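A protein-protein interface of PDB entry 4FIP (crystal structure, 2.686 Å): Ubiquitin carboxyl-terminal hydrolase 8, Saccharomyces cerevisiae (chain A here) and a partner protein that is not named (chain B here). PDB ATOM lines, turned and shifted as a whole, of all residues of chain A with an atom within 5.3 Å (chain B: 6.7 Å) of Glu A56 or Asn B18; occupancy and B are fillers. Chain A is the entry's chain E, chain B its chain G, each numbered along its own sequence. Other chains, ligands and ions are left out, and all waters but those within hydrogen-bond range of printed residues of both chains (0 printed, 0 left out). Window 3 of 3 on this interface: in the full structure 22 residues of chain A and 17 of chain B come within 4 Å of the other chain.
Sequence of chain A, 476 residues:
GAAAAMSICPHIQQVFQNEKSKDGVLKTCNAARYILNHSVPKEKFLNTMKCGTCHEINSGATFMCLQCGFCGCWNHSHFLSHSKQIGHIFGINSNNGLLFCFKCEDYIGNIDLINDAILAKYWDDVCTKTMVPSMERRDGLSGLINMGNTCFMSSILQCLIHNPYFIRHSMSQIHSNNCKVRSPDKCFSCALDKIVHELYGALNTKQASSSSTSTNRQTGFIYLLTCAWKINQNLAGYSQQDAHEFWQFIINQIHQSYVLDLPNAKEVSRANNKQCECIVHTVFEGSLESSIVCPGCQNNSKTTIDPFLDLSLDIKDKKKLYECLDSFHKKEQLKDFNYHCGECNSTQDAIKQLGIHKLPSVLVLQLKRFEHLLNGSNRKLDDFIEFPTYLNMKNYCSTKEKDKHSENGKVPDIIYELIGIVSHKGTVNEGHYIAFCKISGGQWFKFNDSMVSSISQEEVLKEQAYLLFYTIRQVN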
ATOM      1  N   MET A  49      33.314  22.348 -18.331  1.00  0.00           N
ATOM      2  CA  MET A  49      32.657  21.739 -19.496  1.00  0.00           C
ATOM      3  C   MET A  49      33.503  21.696 -20.785  1.00  0.00           C
ATOM      4  O   MET A  49      33.028  21.179 -21.807  1.00  0.00           O
ATOM      5  CB  MET A  49      31.316  22.426 -19.753  1.00  0.00           C
ATOM      6  CG  MET A  49      30.186  21.935 -18.845  1.00  0.00           C
ATOM      7  SD  MET A  49      28.942  23.186 -18.452  1.00  0.00           S
ATOM      8  CE  MET A  49      28.086  22.489 -17.035  1.00  0.00           C
ATOM      9  N   LYS A  50      34.739  22.211 -20.735  1.00  0.00           N
ATOM     10  CA  LYS A  50      35.672  22.148 -21.871  1.00  0.00           C
ATOM     11  C   LYS A  50      36.503  20.846 -21.817  1.00  0.00           C
ATOM     12  O   LYS A  50      37.223  20.614 -20.835  1.00  0.00           O
ATOM     13  CB  LYS A  50      36.600  23.379 -21.838  1.00  0.00           C
ATOM     14  CG  LYS A  50      37.539  23.599 -23.055  1.00  0.00           C
ATOM     15  CD  LYS A  50      38.377  24.882 -22.895  1.00  0.00           C
ATOM     16  CE  LYS A  50      39.073  25.315 -24.175  1.00  0.00           C
ATOM     17  NZ  LYS A  50      38.178  26.024 -25.147  1.00  0.00           N
ATOM     18  N   CYS A  51      36.413  20.001 -22.854  1.00  0.00           N
ATOM     19  CA  CYS A  51      37.196  18.733 -22.905  1.00  0.00           C
ATOM     20  C   CYS A  51      38.701  18.928 -23.102  1.00  0.00           C
ATOM     21  O   CYS A  51      39.095  19.658 -23.961  1.00  0.00           O
ATOM     22  CB  CYS A  51      36.687  17.833 -24.019  1.00  0.00           C
ATOM     23  SG  CYS A  51      37.819  16.504 -24.493  1.00  0.00           S
ATOM     24  N   CYS A  54      40.059  17.287 -26.770  1.00  0.00           N
ATOM     25  CA  CYS A  54      39.506  17.957 -27.982  1.00  0.00           C
ATOM     26  C   CYS A  54      39.160  19.458 -27.863  1.00  0.00           C
ATOM     27  O   CYS A  54      38.945  20.118 -28.870  1.00  0.00           O
ATOM     28  CB  CYS A  54      38.248  17.227 -28.444  1.00  0.00           C
ATOM     29  SG  CYS A  54      36.875  17.412 -27.289  1.00  0.00           S
ATOM     30  N   HIS A  55      39.069  19.974 -26.640  1.00  0.00           N
ATOM     31  CA  HIS A  55      38.890  21.429 -26.352  1.00  0.00           C
ATOM     32  C   HIS A  55      37.513  22.005 -26.625  1.00  0.00           C
ATOM     33  O   HIS A  55      37.293  23.214 -26.489  1.00  0.00           O
ATOM     34  CB  HIS A  55      39.989  22.261 -27.003  1.00  0.00           C
ATOM     35  CG  HIS A  55      41.378  21.867 -26.567  1.00  0.00           C
ATOM     36  ND1 HIS A  55      42.219  22.733 -25.979  1.00  0.00           N
ATOM     37  CD2 HIS A  55      42.064  20.657 -26.666  1.00  0.00           C
ATOM     38  CE1 HIS A  55      43.390  22.118 -25.724  1.00  0.00           C
ATOM     39  NE2 HIS A  55      43.290  20.847 -26.142  1.00  0.00           N
ATOM     40  N   GLU A  56      36.568  21.120 -26.940  1.00  0.00           N
ATOM     41  CA  GLU A  56      35.181  21.484 -27.131  1.00  0.00           C
ATOM     42  C   GLU A  56      34.411  21.576 -25.813  1.00  0.00           C
ATOM     43  O   GLU A  56      34.585  20.758 -24.896  1.00  0.00           O
ATOM     44  CB  GLU A  56      34.473  20.449 -27.999  1.00  0.00           C
ATOM     45  CG  GLU A  56      35.002  20.284 -29.410  1.00  0.00           C
ATOM     46  CD  GLU A  56      34.357  19.091 -30.092  1.00  0.00           C
ATOM     47  OE1 GLU A  56      33.117  19.099 -30.274  1.00  0.00           O
ATOM     48  OE2 GLU A  56      35.093  18.125 -30.411  1.00  0.00           O
ATOM     49  N   ILE A  57      33.519  22.563 -25.772  1.00  0.00           N
ATOM     50  CA  ILE A  57      32.594  22.775 -24.676  1.00  0.00           C
ATOM     51  C   ILE A  57      31.360  21.969 -24.963  1.00  0.00           C
ATOM     52  O   ILE A  57      30.814  22.030 -26.056  1.00  0.00           O
ATOM     53  CB  ILE A  57      32.180  24.259 -24.572  1.00  0.00           C
ATOM     54  CG1 ILE A  57      33.398  25.195 -24.681  1.00  0.00           C
ATOM     55  CG2 ILE A  57      31.406  24.509 -23.290  1.00  0.00           C
ATOM     56  CD1 ILE A  57      34.682  24.605 -24.151  1.00  0.00           C
ATOM     57  N   ASN A  58      30.907  21.216 -23.977  1.00  0.00           N
ATOM     58  CA  ASN A  58      29.716  20.394 -24.138  1.00  0.00           C
ATOM     59  C   ASN A  58      29.794  19.383 -25.275  1.00  0.00           C
ATOM     60  O   ASN A  58      28.826  19.225 -25.991  1.00  0.00           O
ATOM     61  CB  ASN A  58      28.451  21.268 -24.327  1.00  0.00           C
ATOM     62  CG  ASN A  58      28.129  22.106 -23.106  1.00  0.00           C
ATOM     63  OD1 ASN A  58      28.121  21.614 -21.967  1.00  0.00           O
ATOM     64  ND2 ASN A  58      27.880  23.381 -23.333  1.00  0.00           N
ATOM     65  N   SER A  59      30.903  18.660 -25.423  1.00  0.00           N
ATOM     66  CA  SER A  59      30.906  17.503 -26.329  1.00  0.00           C
ATOM     67  C   SER A  59      30.190  16.354 -25.617  1.00  0.00           C
ATOM     68  O   SER A  59      30.695  15.251 -25.499  1.00  0.00           O
ATOM     69  CB  SER A  59      32.329  17.125 -26.777  1.00  0.00           C
ATOM     70  OG  SER A  59      32.345  15.923 -27.551  1.00  0.00           O
ATOM     71  N   GLY A  60      28.970  16.631 -25.174  1.00  0.00           N
ATOM     72  CA  GLY A  60      28.285  15.783 -24.192  1.00  0.00           C
ATOM     73  C   GLY A  60      28.683  16.050 -22.743  1.00  0.00           C
ATOM     74  O   GLY A  60      29.245  17.092 -22.399  1.00  0.00           O
ATOM     75  N   ASN A  75      31.260  12.253 -25.793  1.00  0.00           N
ATOM     76  CA  ASN A  75      30.937  11.897 -27.170  1.00  0.00           C
ATOM     77  C   ASN A  75      32.142  11.404 -27.974  1.00  0.00           C
ATOM     78  O   ASN A  75      31.989  10.524 -28.799  1.00  0.00           O
ATOM     79  CB  ASN A  75      30.228  13.062 -27.892  1.00  0.00           C
ATOM     80  CG  ASN A  75      28.801  13.283 -27.402  1.00  0.00           C
ATOM     81  OD1 ASN A  75      28.386  14.421 -27.240  1.00  0.00           O
ATOM     82  ND2 ASN A  75      28.038  12.201 -27.195  1.00  0.00           N
ATOM     83  N   HIS A  76      33.333  11.934 -27.725  1.00  0.00           N
ATOM     84  CA  HIS A  76      34.556  11.395 -28.386  1.00  0.00           C
ATOM     85  C   HIS A  76      35.394  10.551 -27.454  1.00  0.00           C
ATOM     86  O   HIS A  76      36.618  10.580 -27.487  1.00  0.00           O
ATOM     87  CB  HIS A  76      35.373  12.530 -28.976  1.00  0.00           C
ATOM     88  CG  HIS A  76      34.584  13.402 -29.908  1.00  0.00           C
ATOM     89  ND1 HIS A  76      34.693  14.749 -29.916  1.00  0.00           N
ATOM     90  CD2 HIS A  76      33.608  13.077 -30.846  1.00  0.00           C
ATOM     91  CE1 HIS A  76      33.853  15.254 -30.840  1.00  0.00           C
ATOM     92  NE2 HIS A  76      33.187  14.231 -31.403  1.00  0.00           N
ATOM     93  N   ASN B  13      24.962  23.186 -36.631  1.00  0.00           N
ATOM     94  CA  ASN B  13      24.411  21.866 -36.287  1.00  0.00           C
ATOM     95  C   ASN B  13      25.237  21.187 -35.201  1.00  0.00           C
ATOM     96  O   ASN B  13      24.703  20.538 -34.323  1.00  0.00           O
ATOM     97  CB  ASN B  13      24.310  20.948 -37.505  1.00  0.00           C
ATOM     98  CG  ASN B  13      23.138  21.296 -38.410  1.00  0.00           C
ATOM     99  OD1 ASN B  13      22.021  21.520 -37.949  1.00  0.00           O
ATOM    100  ND2 ASN B  13      23.393  21.327 -39.716  1.00  0.00           N
ATOM    101  N   GLY B  14      26.546  21.352 -35.258  1.00  0.00           N
ATOM    102  CA  GLY B  14      27.422  20.756 -34.261  1.00  0.00           C
ATOM    103  C   GLY B  14      27.258  21.332 -32.869  1.00  0.00           C
ATOM    104  O   GLY B  14      27.465  20.617 -31.882  1.00  0.00           O
ATOM    105  N   ILE B  15      26.896  22.617 -32.783  1.00  0.00           N
ATOM    106  CA  ILE B  15      26.790  23.289 -31.488  1.00  0.00           C
ATOM    107  C   ILE B  15      25.464  22.996 -30.833  1.00  0.00           C
ATOM    108  O   ILE B  15      25.391  22.848 -29.607  1.00  0.00           O
ATOM    109  CB  ILE B  15      26.921  24.805 -31.594  1.00  0.00           C
ATOM    110  CG1 ILE B  15      28.365  25.176 -31.922  1.00  0.00           C
ATOM    111  CG2 ILE B  15      26.493  25.437 -30.278  1.00  0.00           C
ATOM    112  CD1 ILE B  15      28.671  26.650 -31.754  1.00  0.00           C
ATOM    113  N   LEU B  16      24.423  22.950 -31.654  1.00  0.00           N
ATOM    114  CA  LEU B  16      23.097  22.513 -31.215  1.00  0.00           C
ATOM    115  C   LEU B  16      23.177  21.071 -30.737  1.00  0.00           C
ATOM    116  O   LEU B  16      22.688  20.725 -29.646  1.00  0.00           O
ATOM    117  CB  LEU B  16      22.093  22.633 -32.361  1.00  0.00           C
ATOM    118  CG  LEU B  16      20.697  22.031 -32.233  1.00  0.00           C
ATOM    119  CD1 LEU B  16      19.908  22.778 -31.166  1.00  0.00           C
ATOM    120  CD2 LEU B  16      19.971  22.048 -33.576  1.00  0.00           C
ATOM    121  N   ASN B  17      23.829  20.254 -31.553  1.00  0.00           N
ATOM    122  CA  ASN B  17      24.032  18.855 -31.240  1.00  0.00           C
ATOM    123  C   ASN B  17      24.700  18.686 -29.890  1.00  0.00           C
ATOM    124  O   ASN B  17      24.322  17.827 -29.097  1.00  0.00           O
ATOM    125  CB  ASN B  17      24.889  18.168 -32.314  1.00  0.00           C
ATOM    126  CG  ASN B  17      24.810  16.664 -32.226  1.00  0.00           C
ATOM    127  OD1 ASN B  17      23.741  16.116 -31.969  1.00  0.00           O
ATOM    128  ND2 ASN B  17      25.934  15.985 -32.436  1.00  0.00           N
ATOM    129  N   ASN B  18      25.696  19.516 -29.630  1.00  0.00           N
ATOM    130  CA  ASN B  18      26.449  19.406 -28.390  1.00  0.00           C
ATOM    131  C   ASN B  18      25.569  19.722 -27.201  1.00  0.00           C
ATOM    132  O   ASN B  18      25.601  18.992 -26.200  1.00  0.00           O
ATOM    133  CB  ASN B  18      27.674  20.318 -28.421  1.00  0.00           C
ATOM    134  CG  ASN B  18      28.862  19.677 -29.132  1.00  0.00           C
ATOM    135  OD1 ASN B  18      29.990  20.107 -28.948  1.00  0.00           O
ATOM    136  ND2 ASN B  18      28.604  18.634 -29.941  1.00  0.00           N
ATOM    137  N   LEU B  19      24.753  20.777 -27.330  1.00  0.00           N
ATOM    138  CA  LEU B  19      23.859  21.190 -26.247  1.00  0.00           C
ATOM    139  C   LEU B  19      22.780  20.159 -25.965  1.00  0.00           C
ATOM    140  O   LEU B  19      22.487  19.881 -24.800  1.00  0.00           O
ATOM    141  CB  LEU B  19      23.212  22.545 -26.542  1.00  0.00           C
ATOM    142  CG  LEU B  19      24.164  23.722 -26.478  1.00  0.00           C
ATOM    143  CD1 LEU B  19      23.508  24.993 -26.992  1.00  0.00           C
ATOM    144  CD2 LEU B  19      24.667  23.902 -25.064  1.00  0.00           C
ATOM    145  N   LEU B  20      22.178  19.618 -27.020  1.00  0.00           N
ATOM    146  CA  LEU B  20      21.122  18.608 -26.871  1.00  0.00           C
ATOM    147  C   LEU B  20      21.686  17.382 -26.163  1.00  0.00           C
ATOM    148  O   LEU B  20      21.214  16.992 -25.085  1.00  0.00           O
ATOM    149  CB  LEU B  20      20.560  18.167 -28.232  1.00  0.00           C
ATOM    150  CG  LEU B  20      19.694  19.143 -29.010  1.00  0.00           C
ATOM    151  CD1 LEU B  20      19.265  18.557 -30.345  1.00  0.00           C
ATOM    152  CD2 LEU B  20      18.497  19.500 -28.146  1.00  0.00           C
ATOM    153  N   THR B  21      22.722  16.796 -26.756  1.00  0.00           N
ATOM    154  CA  THR B  21      23.331  15.602 -26.197  1.00  0.00           C
ATOM    155  C   THR B  21      23.779  15.811 -24.750  1.00  0.00           C
ATOM    156  O   THR B  21      23.480  14.965 -23.908  1.00  0.00           O
ATOM    157  CB  THR B  21      24.524  15.149 -27.035  1.00  0.00           C
ATOM    158  OG1 THR B  21      25.370  16.280 -27.248  1.00  0.00           O
ATOM    159  CG2 THR B  21      24.048  14.548 -28.387  1.00  0.00           C
ATOM    160  N   THR B  22      24.479  16.912 -24.454  1.00  0.00           N
ATOM    161  CA  THR B  22      24.871  17.197 -23.058  1.00  0.00           C
ATOM    162  C   THR B  22      23.635  17.170 -22.149  1.00  0.00           C
ATOM    163  O   THR B  22      23.635  16.550 -21.074  1.00  0.00           O
ATOM    164  CB  THR B  22      25.567  18.562 -22.913  1.00  0.00           C
ATOM    165  OG1 THR B  22      26.867  18.491 -23.513  1.00  0.00           O
ATOM    166  CG2 THR B  22      25.721  18.943 -21.449  1.00  0.00           C
ATOM    167  N   LEU B  23      22.573  17.810 -22.641  1.00  0.00           N
ATOM    168  CA  LEU B  23      21.312  17.910 -21.927  1.00  0.00           C
ATOM    169  C   LEU B  23      20.635  16.550 -21.784  1.00  0.00           C
ATOM    170  O   LEU B  23      20.292  16.152 -20.673  1.00  0.00           O
ATOM    171  CB  LEU B  23      20.386  18.918 -22.608  1.00  0.00           C
ATOM    172  CG  LEU B  23      19.023  19.131 -21.948  1.00  0.00           C
ATOM    173  CD1 LEU B  23      19.135  19.458 -20.453  1.00  0.00           C
ATOM    174  CD2 LEU B  23      18.249  20.200 -22.703  1.00  0.00           C
ATOM    175  N   GLN B  25      21.911  13.658 -21.823  1.00  0.00           N
ATOM    176  CA  GLN B  25      22.739  12.832 -20.954  1.00  0.00           C
ATOM    177  C   GLN B  25      22.601  13.208 -19.490  1.00  0.00           C
ATOM    178  O   GLN B  25      22.658  12.340 -18.639  1.00  0.00           O
ATOM    179  CB  GLN B  25      24.195  12.945 -21.363  1.00  0.00           C
ATOM    180  CG  GLN B  25      24.504  12.227 -22.657  1.00  0.00           C
ATOM    181  CD  GLN B  25      25.925  12.479 -23.124  1.00  0.00           C
ATOM    182  OE1 GLN B  25      26.166  12.648 -24.318  1.00  0.00           O
ATOM    183  NE2 GLN B  25      26.873  12.495 -22.183  1.00  0.00           N
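Among the printed residues, 10 pairs touch across the chains. Among the printed residues, no Asp or Glu carboxylate lies within 4 Å of a Lys or Arg side-chain nitrogen of the other chain.
Among the printed residues, pairs that only touch across the chains: Asn A75 with Thr B21, Glu A56 with Asn B18, Ile A57 with Asn B18, Asn A58 with Leu B19, Gly A60 with Gln B25 and Ser A59 with Asn B18.
O of Asn B17 lies within hydrogen-bond range of OG1 of Thr B21 (2.6 Å). The backbone carbonyl oxygen of Asn B18 lies within hydrogen-bond range of the side-chain hydroxyl of Thr B21 (2.9 Å). The backbone carbonyl oxygen (O) of Met A49 lies within hydrogen-bond range of the backbone NH (N) of Asn A58, 3.0 Å away. N of Gly A60 sits at hydrogen-bond distance from OD1 of Asn A75 (3.1 Å). The backbone carbonyl oxygen of Gly B14 lies within hydrogen-bond range of the side-chain amide nitrogen of Asn B18 (3.0 Å). OE2 of Glu A56 sits close to SG of Cys A54 (3.7 Å).
The backbone carbonyl oxygen (O) of Asn A58 lies close to the side-chain amide oxygen (OD1) of Asn B18 (3.3 Å). The backbone carbonyl oxygen (O) of Asn A58 sits at hydrogen-bond distance from the side-chain hydroxyl (OG1) of Thr B22 (3.2 Å). The backbone carbonyl oxygen (O) of Gly A60 lies within hydrogen-bond range of the side-chain hydroxyl (OG1) of Thr B22. The side-chain amide nitrogen of Asn A75 sits at hydrogen-bond distance from the side-chain amide oxygen of Gln B25, 3.5 Å away.
Of chain B, only Asn B18 comes within 4 Å of Glu A56. Of the printed residues of chain B, Asn A75 touches Thr B21 and Gln B25. Asn B18 touches just these residues of chain A: Glu A56, Ile A57, Asn A58 and Ser A59. Printed residues of chain A within 4 Å of Leu B19: Asn A58. Of the printed residues of chain A, Thr B22 touches Asn A58 (3.2 Å) and Gly A60 (3.0 Å). The nearest residue of chain B that does not touch Glu A56 is Gly B14 (6.1 Å). The nearest residue of chain A that does not touch Asn B18 is Gly A60 (4.2 Å). The nearest printed residue of chain A that does not touch Thr B22 is Ser A59 (4.5 Å).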
